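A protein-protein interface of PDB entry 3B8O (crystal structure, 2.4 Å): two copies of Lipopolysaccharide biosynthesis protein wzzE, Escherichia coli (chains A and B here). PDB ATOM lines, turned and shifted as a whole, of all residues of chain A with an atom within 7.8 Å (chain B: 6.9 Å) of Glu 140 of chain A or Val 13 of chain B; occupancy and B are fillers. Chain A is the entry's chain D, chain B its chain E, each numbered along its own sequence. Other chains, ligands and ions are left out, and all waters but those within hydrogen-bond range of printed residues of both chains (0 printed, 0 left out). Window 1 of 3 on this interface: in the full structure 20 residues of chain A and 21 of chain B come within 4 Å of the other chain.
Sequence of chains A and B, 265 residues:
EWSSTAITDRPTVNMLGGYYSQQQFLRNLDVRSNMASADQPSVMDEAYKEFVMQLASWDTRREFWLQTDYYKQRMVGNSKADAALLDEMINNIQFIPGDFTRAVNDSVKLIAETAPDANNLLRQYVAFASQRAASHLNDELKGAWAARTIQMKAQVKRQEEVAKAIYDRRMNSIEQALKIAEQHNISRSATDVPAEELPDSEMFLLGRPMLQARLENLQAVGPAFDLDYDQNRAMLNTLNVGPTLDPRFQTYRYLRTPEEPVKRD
The side-chain carboxylate (OE2) of Glu 140 of chain A sits close to the side-chain amide oxygen (OD1) of Asn 14 of chain B, 3.3 Å away.
The side-chain carboxylate of Glu 140 of chain A lies within hydrogen-bond range of the backbone NH of Val 13 of chain B, at 2.5 Å.
OE2 of Glu 50 of chain A lies within salt-bridge range of NH1 of Arg 253 of chain B, 3.0 Å away.
The backbone carbonyl oxygen (O) of Asp 139 of chain A sits close to the side-chain amide oxygen (OD1) of Asn 14 of chain B, 3.0 Å away.
No position is printed for both chains.
Of the 7 pairs that touch across the chains among the printed residues, none has its exchanged pair printed and touching as well.
Of the 12 printed residues of chain B, 4 touch a printed residue of chain A.
Printed residues of chain B that touch a printed residue of chain A: Thr 12, Val 13, Asn 14 and Arg 253.
Along chain B the printed residues that touch a printed residue of chain A span positions 12 to 253.
Of the 20 printed residues of chain A, 4 touch a printed residue of chain B.
Hydrophobic or aromatic side chains of chain A that line the printed part of chain B: His 136.
Among the printed residues, 7 pairs touch across the chains.
The side-chain carboxylate (OE1) of Glu 50 of chain A is in hydrogen-bond range of a ring nitrogen (ND1) of His 136 of chain A (3.3 Å).
The side-chain hydroxyl (OG1) of Thr 12 of chain B sits at hydrogen-bond distance from the side-chain amide nitrogen (ND2) of Asn 14 of chain B.
His 136 of chain A touches Thr 12 of chain B (NE2 to CG2, 2.9 Å).
Arg 253 of chain B touches His 136 of chain A (NH1 to CD2, 3.6 Å).
CB of Thr 12 of chain B touches OE2 of Glu 140 of chain A, 3.0 Å away.
Of chain B, only Thr 12, Val 13 and Asn 14 come within 4 Å of Glu 140 of chain A.
Of chain A, only Glu 140 comes within 4 Å of Val 13 of chain B.
Of the printed residues of chain A, Arg 253 of chain B touches Glu 50 (2.4 Å) and His 136 (3.6 Å).
Printed residues of chain A within 4 Å of Asn 14 of chain B: Asp 139 (3.0 Å) and Glu 140 (3.3 Å).
The nearest residue of chain A that does not touch Val 13 of chain B is Gly 143 of chain A (4.3 Å).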
ATOM      1  N   TYR A  19     -13.858  31.231 -28.193  1.00  0.00           N
ATOM      2  CA  TYR A  19     -15.250  31.446 -27.843  1.00  0.00           C
ATOM      3  C   TYR A  19     -15.714  32.866 -28.098  1.00  0.00           C
ATOM      4  O   TYR A  19     -16.876  33.082 -28.467  1.00  0.00           O
ATOM      5  CB  TYR A  19     -15.503  31.096 -26.377  1.00  0.00           C
ATOM      6  CG  TYR A  19     -16.879  31.472 -25.894  1.00  0.00           C
ATOM      7  CD1 TYR A  19     -17.990  30.678 -26.197  1.00  0.00           C
ATOM      8  CD2 TYR A  19     -17.077  32.617 -25.147  1.00  0.00           C
ATOM      9  CE1 TYR A  19     -19.265  31.020 -25.745  1.00  0.00           C
ATOM     10  CE2 TYR A  19     -18.349  32.970 -24.686  1.00  0.00           C
ATOM     11  CZ  TYR A  19     -19.423  32.172 -24.980  1.00  0.00           C
ATOM     12  OH  TYR A  19     -20.662  32.543 -24.535  1.00  0.00           O
ATOM     13  N   GLN A  23     -18.990  34.227 -30.298  1.00  0.00           N
ATOM     14  CA  GLN A  23     -20.156  34.795 -29.674  1.00  0.00           C
ATOM     15  C   GLN A  23     -20.410  36.154 -30.324  1.00  0.00           C
ATOM     16  O   GLN A  23     -21.568  36.549 -30.559  1.00  0.00           O
ATOM     17  CB  GLN A  23     -19.947  34.861 -28.148  1.00  0.00           C
ATOM     18  CG  GLN A  23     -21.157  35.212 -27.298  1.00  0.00           C
ATOM     19  CD  GLN A  23     -22.327  34.254 -27.440  1.00  0.00           C
ATOM     20  OE1 GLN A  23     -22.172  33.106 -27.867  1.00  0.00           O
ATOM     21  NE2 GLN A  23     -23.519  34.730 -27.065  1.00  0.00           N
ATOM     22  N   LEU A  26     -22.039  35.715 -33.759  1.00  0.00           N
ATOM     23  CA  LEU A  26     -23.484  35.562 -33.581  1.00  0.00           C
ATOM     24  C   LEU A  26     -24.172  36.850 -33.158  1.00  0.00           C
ATOM     25  O   LEU A  26     -25.360  37.005 -33.384  1.00  0.00           O
ATOM     26  CB  LEU A  26     -23.856  34.441 -32.602  1.00  0.00           C
ATOM     27  CG  LEU A  26     -23.625  32.985 -33.002  1.00  0.00           C
ATOM     28  CD1 LEU A  26     -24.117  32.097 -31.878  1.00  0.00           C
ATOM     29  CD2 LEU A  26     -24.273  32.559 -34.337  1.00  0.00           C
ATOM     30  N   GLU A  50     -22.168  33.484 -15.771  1.00  0.00           N
ATOM     31  CA  GLU A  50     -22.407  32.077 -15.663  1.00  0.00           C
ATOM     32  C   GLU A  50     -21.450  31.478 -14.626  1.00  0.00           C
ATOM     33  O   GLU A  50     -21.814  30.572 -13.820  1.00  0.00           O
ATOM     34  CB  GLU A  50     -22.228  31.427 -17.034  1.00  0.00           C
ATOM     35  CG  GLU A  50     -22.337  29.922 -17.029  1.00  0.00           C
ATOM     36  CD  GLU A  50     -23.728  29.388 -16.634  1.00  0.00           C
ATOM     37  OE1 GLU A  50     -24.758  30.028 -16.976  1.00  0.00           O
ATOM     38  OE2 GLU A  50     -23.786  28.301 -16.021  1.00  0.00           O
ATOM     39  N   ALA A 133     -18.906  26.389 -16.275  1.00  0.00           N
ATOM     40  CA  ALA A 133     -19.395  27.572 -16.948  1.00  0.00           C
ATOM     41  C   ALA A 133     -19.028  27.510 -18.422  1.00  0.00           C
ATOM     42  O   ALA A 133     -19.872  27.802 -19.287  1.00  0.00           O
ATOM     43  CB  ALA A 133     -18.844  28.843 -16.305  1.00  0.00           C
ATOM     44  N   ALA A 134     -17.784  27.111 -18.699  1.00  0.00           N
ATOM     45  CA  ALA A 134     -17.312  26.981 -20.067  1.00  0.00           C
ATOM     46  C   ALA A 134     -18.158  26.002 -20.883  1.00  0.00           C
ATOM     47  O   ALA A 134     -18.565  26.359 -21.978  1.00  0.00           O
ATOM     48  CB  ALA A 134     -15.837  26.626 -20.123  1.00  0.00           C
ATOM     49  N   SER A 135     -18.445  24.806 -20.350  1.00  0.00           N
ATOM     50  CA  SER A 135     -19.263  23.834 -21.074  1.00  0.00           C
ATOM     51  C   SER A 135     -20.682  24.352 -21.264  1.00  0.00           C
ATOM     52  O   SER A 135     -21.313  24.100 -22.297  1.00  0.00           O
ATOM     53  CB  SER A 135     -19.305  22.460 -20.382  1.00  0.00           C
ATOM     54  OG  SER A 135     -18.004  22.063 -19.969  1.00  0.00           O
ATOM     55  N   HIS A 136     -21.181  25.086 -20.274  1.00  0.00           N
ATOM     56  CA  HIS A 136     -22.520  25.604 -20.397  1.00  0.00           C
ATOM     57  C   HIS A 136     -22.581  26.668 -21.474  1.00  0.00           C
ATOM     58  O   HIS A 136     -23.443  26.611 -22.329  1.00  0.00           O
ATOM     59  CB  HIS A 136     -23.080  26.159 -19.098  1.00  0.00           C
ATOM     60  CG  HIS A 136     -24.432  26.754 -19.295  1.00  0.00           C
ATOM     61  ND1 HIS A 136     -24.620  28.091 -19.594  1.00  0.00           N
ATOM     62  CD2 HIS A 136     -25.651  26.168 -19.387  1.00  0.00           C
ATOM     63  CE1 HIS A 136     -25.904  28.308 -19.816  1.00  0.00           C
ATOM     64  NE2 HIS A 136     -26.547  27.158 -19.705  1.00  0.00           N
ATOM     65  N   LEU A 137     -21.667  27.636 -21.437  1.00  0.00           N
ATOM     66  CA  LEU A 137     -21.588  28.656 -22.483  1.00  0.00           C
ATOM     67  C   LEU A 137     -21.426  28.060 -23.907  1.00  0.00           C
ATOM     68  O   LEU A 137     -22.062  28.523 -24.854  1.00  0.00           O
ATOM     69  CB  LEU A 137     -20.472  29.644 -22.177  1.00  0.00           C
ATOM     70  CG  LEU A 137     -20.735  30.504 -20.944  1.00  0.00           C
ATOM     71  CD1 LEU A 137     -19.413  30.988 -20.306  1.00  0.00           C
ATOM     72  CD2 LEU A 137     -21.695  31.663 -21.233  1.00  0.00           C
ATOM     73  N   ASN A 138     -20.620  27.016 -24.040  1.00  0.00           N
ATOM     74  CA  ASN A 138     -20.557  26.277 -25.293  1.00  0.00           C
ATOM     75  C   ASN A 138     -21.855  25.572 -25.740  1.00  0.00           C
ATOM     76  O   ASN A 138     -22.096  25.468 -26.913  1.00  0.00           O
ATOM     77  CB  ASN A 138     -19.358  25.333 -25.337  1.00  0.00           C
ATOM     78  CG  ASN A 138     -18.058  26.067 -25.603  1.00  0.00           C
ATOM     79  OD1 ASN A 138     -16.994  25.497 -25.491  1.00  0.00           O
ATOM     80  ND2 ASN A 138     -18.142  27.334 -25.946  1.00  0.00           N
ATOM     81  N   ASP A 139     -22.659  25.088 -24.806  1.00  0.00           N
ATOM     82  CA  ASP A 139     -24.009  24.604 -25.110  1.00  0.00           C
ATOM     83  C   ASP A 139     -24.944  25.737 -25.561  1.00  0.00           C
ATOM     84  O   ASP A 139     -25.769  25.543 -26.443  1.00  0.00           O
ATOM     85  CB  ASP A 139     -24.624  23.883 -23.894  1.00  0.00           C
ATOM     86  CG  ASP A 139     -24.039  22.498 -23.672  1.00  0.00           C
ATOM     87  OD1 ASP A 139     -23.203  22.087 -24.507  1.00  0.00           O
ATOM     88  OD2 ASP A 139     -24.415  21.800 -22.684  1.00  0.00           O
ATOM     89  N   GLU A 140     -24.826  26.916 -24.953  1.00  0.00           N
ATOM     90  CA  GLU A 140     -25.628  28.024 -25.408  1.00  0.00           C
ATOM     91  C   GLU A 140     -25.172  28.395 -26.823  1.00  0.00           C
ATOM     92  O   GLU A 140     -26.023  28.618 -27.707  1.00  0.00           O
ATOM     93  CB  GLU A 140     -25.560  29.242 -24.470  1.00  0.00           C
ATOM     94  CG  GLU A 140     -26.487  29.257 -23.262  1.00  0.00           C
ATOM     95  CD  GLU A 140     -27.918  29.774 -23.550  1.00  0.00           C
ATOM     96  OE1 GLU A 140     -28.307  30.904 -23.117  1.00  0.00           O
ATOM     97  OE2 GLU A 140     -28.672  29.021 -24.203  1.00  0.00           O
ATOM     98  N   LEU A 141     -23.849  28.442 -27.039  1.00  0.00           N
ATOM     99  CA  LEU A 141     -23.302  28.763 -28.367  1.00  0.00           C
ATOM    100  C   LEU A 141     -23.817  27.792 -29.449  1.00  0.00           C
ATOM    101  O   LEU A 141     -24.569  28.199 -30.316  1.00  0.00           O
ATOM    102  CB  LEU A 141     -21.761  28.823 -28.359  1.00  0.00           C
ATOM    103  CG  LEU A 141     -20.939  29.225 -29.603  1.00  0.00           C
ATOM    104  CD1 LEU A 141     -21.263  30.620 -30.089  1.00  0.00           C
ATOM    105  CD2 LEU A 141     -19.463  29.177 -29.278  1.00  0.00           C
ATOM    106  N   LYS A 142     -23.427  26.522 -29.365  1.00  0.00           N
ATOM    107  CA  LYS A 142     -23.869  25.460 -30.266  1.00  0.00           C
ATOM    108  C   LYS A 142     -25.365  25.549 -30.652  1.00  0.00           C
ATOM    109  O   LYS A 142     -25.745  25.326 -31.821  1.00  0.00           O
ATOM    110  CB  LYS A 142     -23.547  24.101 -29.644  1.00  0.00           C
ATOM    111  CG  LYS A 142     -23.950  22.884 -30.485  1.00  0.00           C
ATOM    112  CD  LYS A 142     -23.578  21.572 -29.774  1.00  0.00           C
ATOM    113  CE  LYS A 142     -24.276  20.362 -30.400  1.00  0.00           C
ATOM    114  NZ  LYS A 142     -23.785  19.035 -29.870  1.00  0.00           N
ATOM    115  N   GLY A 143     -26.191  25.899 -29.678  1.00  0.00           N
ATOM    116  CA  GLY A 143     -27.627  26.035 -29.887  1.00  0.00           C
ATOM    117  C   GLY A 143     -28.117  27.390 -30.395  1.00  0.00           C
ATOM    118  O   GLY A 143     -29.245  27.494 -30.919  1.00  0.00           O
ATOM    119  N   ALA A 144     -27.306  28.435 -30.236  1.00  0.00           N
ATOM    120  CA  ALA A 144     -27.692  29.751 -30.719  1.00  0.00           C
ATOM    121  C   ALA A 144     -27.361  29.758 -32.199  1.00  0.00           C
ATOM    122  O   ALA A 144     -28.099  30.290 -33.052  1.00  0.00           O
ATOM    123  CB  ALA A 144     -26.943  30.831 -29.989  1.00  0.00           C
ATOM    124  N   TRP A 145     -26.267  29.086 -32.490  1.00  0.00           N
ATOM    125  CA  TRP A 145     -25.782  28.932 -33.807  1.00  0.00           C
ATOM    126  C   TRP A 145     -26.745  28.053 -34.602  1.00  0.00           C
ATOM    127  O   TRP A 145     -27.082  28.353 -35.747  1.00  0.00           O
ATOM    128  CB  TRP A 145     -24.401  28.293 -33.680  1.00  0.00           C
ATOM    129  CG  TRP A 145     -23.600  28.216 -34.922  1.00  0.00           C
ATOM    130  CD1 TRP A 145     -23.831  27.410 -35.985  1.00  0.00           C
ATOM    131  CD2 TRP A 145     -22.404  28.945 -35.213  1.00  0.00           C
ATOM    132  NE1 TRP A 145     -22.852  27.590 -36.932  1.00  0.00           N
ATOM    133  CE2 TRP A 145     -21.964  28.530 -36.481  1.00  0.00           C
ATOM    134  CE3 TRP A 145     -21.654  29.903 -34.519  1.00  0.00           C
ATOM    135  CZ2 TRP A 145     -20.806  29.048 -37.080  1.00  0.00           C
ATOM    136  CZ3 TRP A 145     -20.499  30.407 -35.112  1.00  0.00           C
ATOM    137  CH2 TRP A 145     -20.091  29.984 -36.379  1.00  0.00           C
ATOM    138  N   ALA A 146     -27.188  26.957 -33.999  1.00  0.00           N
ATOM    139  CA  ALA A 146     -28.137  26.083 -34.650  1.00  0.00           C
ATOM    140  C   ALA A 146     -29.387  26.882 -34.992  1.00  0.00           C
ATOM    141  O   ALA A 146     -29.872  26.799 -36.095  1.00  0.00           O
ATOM    142  CB  ALA A 146     -28.470  24.894 -33.754  1.00  0.00           C
ATOM    143  N   ALA A 147     -29.871  27.687 -34.049  1.00  0.00           N
ATOM    144  CA  ALA A 147     -31.040  28.528 -34.308  1.00  0.00           C
ATOM    145  C   ALA A 147     -30.819  29.538 -35.453  1.00  0.00           C
ATOM    146  O   ALA A 147     -31.660  29.652 -36.321  1.00  0.00           O
ATOM    147  CB  ALA A 147     -31.515  29.239 -33.039  1.00  0.00           C
ATOM    148  N   LEU A 245     -15.982  24.247 -30.567  1.00  0.00           N
ATOM    149  CA  LEU A 245     -16.367  24.187 -29.169  1.00  0.00           C
ATOM    150  C   LEU A 245     -15.201  23.733 -28.307  1.00  0.00           C
ATOM    151  O   LEU A 245     -15.071  22.552 -27.975  1.00  0.00           O
ATOM    152  CB  LEU A 245     -17.611  23.307 -28.993  1.00  0.00           C
ATOM    153  CG  LEU A 245     -18.792  23.616 -29.942  1.00  0.00           C
ATOM    154  CD1 LEU A 245     -19.805  22.467 -29.920  1.00  0.00           C
ATOM    155  CD2 LEU A 245     -19.462  24.961 -29.613  1.00  0.00           C
ATOM    156  N   PRO B  11     -34.254  29.354 -18.233  1.00  0.00           N
ATOM    157  CA  PRO B  11     -33.605  28.267 -18.952  1.00  0.00           C
ATOM    158  C   PRO B  11     -32.658  28.874 -19.942  1.00  0.00           C
ATOM    159  O   PRO B  11     -32.564  30.091 -19.986  1.00  0.00           O
ATOM    160  CB  PRO B  11     -34.774  27.581 -19.669  1.00  0.00           C
ATOM    161  CG  PRO B  11     -35.751  28.662 -19.902  1.00  0.00           C
ATOM    162  CD  PRO B  11     -35.624  29.598 -18.733  1.00  0.00           C
ATOM    163  N   THR B  12     -31.959  28.049 -20.709  1.00  0.00           N
ATOM    164  CA  THR B  12     -31.064  28.537 -21.754  1.00  0.00           C
ATOM    165  C   THR B  12     -31.650  28.199 -23.114  1.00  0.00           C
ATOM    166  O   THR B  12     -32.487  27.307 -23.198  1.00  0.00           O
ATOM    167  CB  THR B  12     -29.688  27.892 -21.644  1.00  0.00           C
ATOM    168  OG1 THR B  12     -29.831  26.440 -21.484  1.00  0.00           O
ATOM    169  CG2 THR B  12     -28.974  28.476 -20.443  1.00  0.00           C
ATOM    170  N   VAL B  13     -31.217  28.909 -24.168  1.00  0.00           N
ATOM    171  CA  VAL B  13     -31.761  28.719 -25.518  1.00  0.00           C
ATOM    172  C   VAL B  13     -31.940  27.249 -25.919  1.00  0.00           C
ATOM    173  O   VAL B  13     -33.050  26.837 -26.326  1.00  0.00           O
ATOM    174  CB  VAL B  13     -30.945  29.440 -26.631  1.00  0.00           C
ATOM    175  CG1 VAL B  13     -31.730  29.445 -27.931  1.00  0.00           C
ATOM    176  CG2 VAL B  13     -30.584  30.861 -26.236  1.00  0.00           C
ATOM    177  N   ASN B  14     -30.835  26.462 -25.811  1.00  0.00           N
ATOM    178  CA  ASN B  14     -30.961  25.016 -26.092  1.00  0.00           C
ATOM    179  C   ASN B  14     -32.117  24.311 -25.362  1.00  0.00           C
ATOM    180  O   ASN B  14     -32.744  23.390 -25.904  1.00  0.00           O
ATOM    181  CB  ASN B  14     -29.648  24.265 -25.793  1.00  0.00           C
ATOM    182  CG  ASN B  14     -28.891  24.854 -24.583  1.00  0.00           C
ATOM    183  OD1 ASN B  14     -28.200  25.842 -24.725  1.00  0.00           O
ATOM    184  ND2 ASN B  14     -28.899  24.275 -23.393  1.00  0.00           N
ATOM    185  N   MET B  15     -32.411  24.747 -24.136  1.00  0.00           N
ATOM    186  CA  MET B  15     -33.458  24.081 -23.365  1.00  0.00           C
ATOM    187  C   MET B  15     -34.862  24.298 -23.922  1.00  0.00           C
ATOM    188  O   MET B  15     -35.775  23.523 -23.616  1.00  0.00           O
ATOM    189  CB  MET B  15     -33.418  24.543 -21.934  1.00  0.00           C
ATOM    190  CG  MET B  15     -32.133  24.208 -21.269  1.00  0.00           C
ATOM    191  SD  MET B  15     -32.577  24.128 -19.386  1.00  0.00           S
ATOM    192  CE  MET B  15     -30.906  25.027 -18.827  1.00  0.00           C
ATOM    193  N   LEU B  16     -35.004  25.342 -24.745  1.00  0.00           N
ATOM    194  CA  LEU B  16     -36.265  25.695 -25.389  1.00  0.00           C
ATOM    195  C   LEU B  16     -36.549  24.935 -26.683  1.00  0.00           C
ATOM    196  O   LEU B  16     -37.687  24.956 -27.163  1.00  0.00           O
ATOM    197  CB  LEU B  16     -36.350  27.197 -25.621  1.00  0.00           C
ATOM    198  CG  LEU B  16     -36.110  28.135 -24.425  1.00  0.00           C
ATOM    199  CD1 LEU B  16     -35.987  29.582 -24.912  1.00  0.00           C
ATOM    200  CD2 LEU B  16     -37.175  28.032 -23.357  1.00  0.00           C
ATOM    201  N   GLY B  17     -35.542  24.248 -27.224  1.00  0.00           N
ATOM    202  CA  GLY B  17     -35.701  23.397 -28.406  1.00  0.00           C
ATOM    203  C   GLY B  17     -36.331  24.163 -29.551  1.00  0.00           C
ATOM    204  O   GLY B  17     -36.157  25.385 -29.662  1.00  0.00           O
ATOM    205  N   GLY B  18     -37.080  23.450 -30.394  1.00  0.00           N
ATOM    206  CA  GLY B  18     -37.857  24.052 -31.478  1.00  0.00           C
ATOM    207  C   GLY B  18     -38.697  25.272 -31.108  1.00  0.00           C
ATOM    208  O   GLY B  18     -39.086  26.036 -32.000  1.00  0.00           O
ATOM    209  N   TYR B  20     -37.842  28.086 -29.393  1.00  0.00           N
ATOM    210  CA  TYR B  20     -37.145  29.365 -29.531  1.00  0.00           C
ATOM    211  C   TYR B  20     -37.189  29.930 -30.959  1.00  0.00           C
ATOM    212  O   TYR B  20     -37.655  31.059 -31.161  1.00  0.00           O
ATOM    213  CB  TYR B  20     -35.708  29.270 -29.041  1.00  0.00           C
ATOM    214  CG  TYR B  20     -34.926  30.559 -29.161  1.00  0.00           C
ATOM    215  CD1 TYR B  20     -35.028  31.558 -28.191  1.00  0.00           C
ATOM    216  CD2 TYR B  20     -34.079  30.773 -30.237  1.00  0.00           C
ATOM    217  CE1 TYR B  20     -34.309  32.733 -28.294  1.00  0.00           C
ATOM    218  CE2 TYR B  20     -33.357  31.945 -30.357  1.00  0.00           C
ATOM    219  CZ  TYR B  20     -33.469  32.921 -29.377  1.00  0.00           C
ATOM    220  OH  TYR B  20     -32.734  34.087 -29.503  1.00  0.00           O
ATOM    221  N   SER B  21     -36.727  29.152 -31.938  1.00  0.00           N
ATOM    222  CA  SER B  21     -36.672  29.639 -33.327  1.00  0.00           C
ATOM    223  C   SER B  21     -38.043  30.060 -33.885  1.00  0.00           C
ATOM    224  O   SER B  21     -38.125  30.978 -34.692  1.00  0.00           O
ATOM    225  CB  SER B  21     -36.006  28.627 -34.255  1.00  0.00           C
ATOM    226  OG  SER B  21     -36.749  27.427 -34.310  1.00  0.00           O
ATOM    227  N   MET B  44     -36.328  33.434 -23.289  1.00  0.00           N
ATOM    228  CA  MET B  44     -36.092  32.601 -22.121  1.00  0.00           C
ATOM    229  C   MET B  44     -36.577  33.244 -20.829  1.00  0.00           C
ATOM    230  O   MET B  44     -36.962  32.548 -19.934  1.00  0.00           O
ATOM    231  CB  MET B  44     -34.664  32.011 -22.035  1.00  0.00           C
ATOM    232  CG  MET B  44     -33.608  32.680 -22.840  1.00  0.00           C
ATOM    233  SD  MET B  44     -33.459  32.434 -24.821  1.00  0.00           S
ATOM    234  CE  MET B  44     -32.338  33.991 -25.127  1.00  0.00           C
ATOM    235  N   ARG B 253     -33.975  26.347 -15.298  1.00  0.00           N
ATOM    236  CA  ARG B 253     -32.903  25.456 -14.892  1.00  0.00           C
ATOM    237  C   ARG B 253     -32.743  25.432 -13.387  1.00  0.00           C
ATOM    238  O   ARG B 253     -33.194  26.336 -12.699  1.00  0.00           O
ATOM    239  CB  ARG B 253     -31.573  25.699 -15.615  1.00  0.00           C
ATOM    240  CG  ARG B 253     -30.828  26.957 -15.287  1.00  0.00           C
ATOM    241  CD  ARG B 253     -29.354  26.709 -15.543  1.00  0.00           C
ATOM    242  NE  ARG B 253     -28.690  27.934 -15.927  1.00  0.00           N
ATOM    243  CZ  ARG B 253     -27.391  28.090 -16.164  1.00  0.00           C
ATOM    244  NH1 ARG B 253     -26.530  27.102 -16.070  1.00  0.00           N
ATOM    245  NH2 ARG B 253     -26.959  29.272 -16.518  1.00  0.00           N
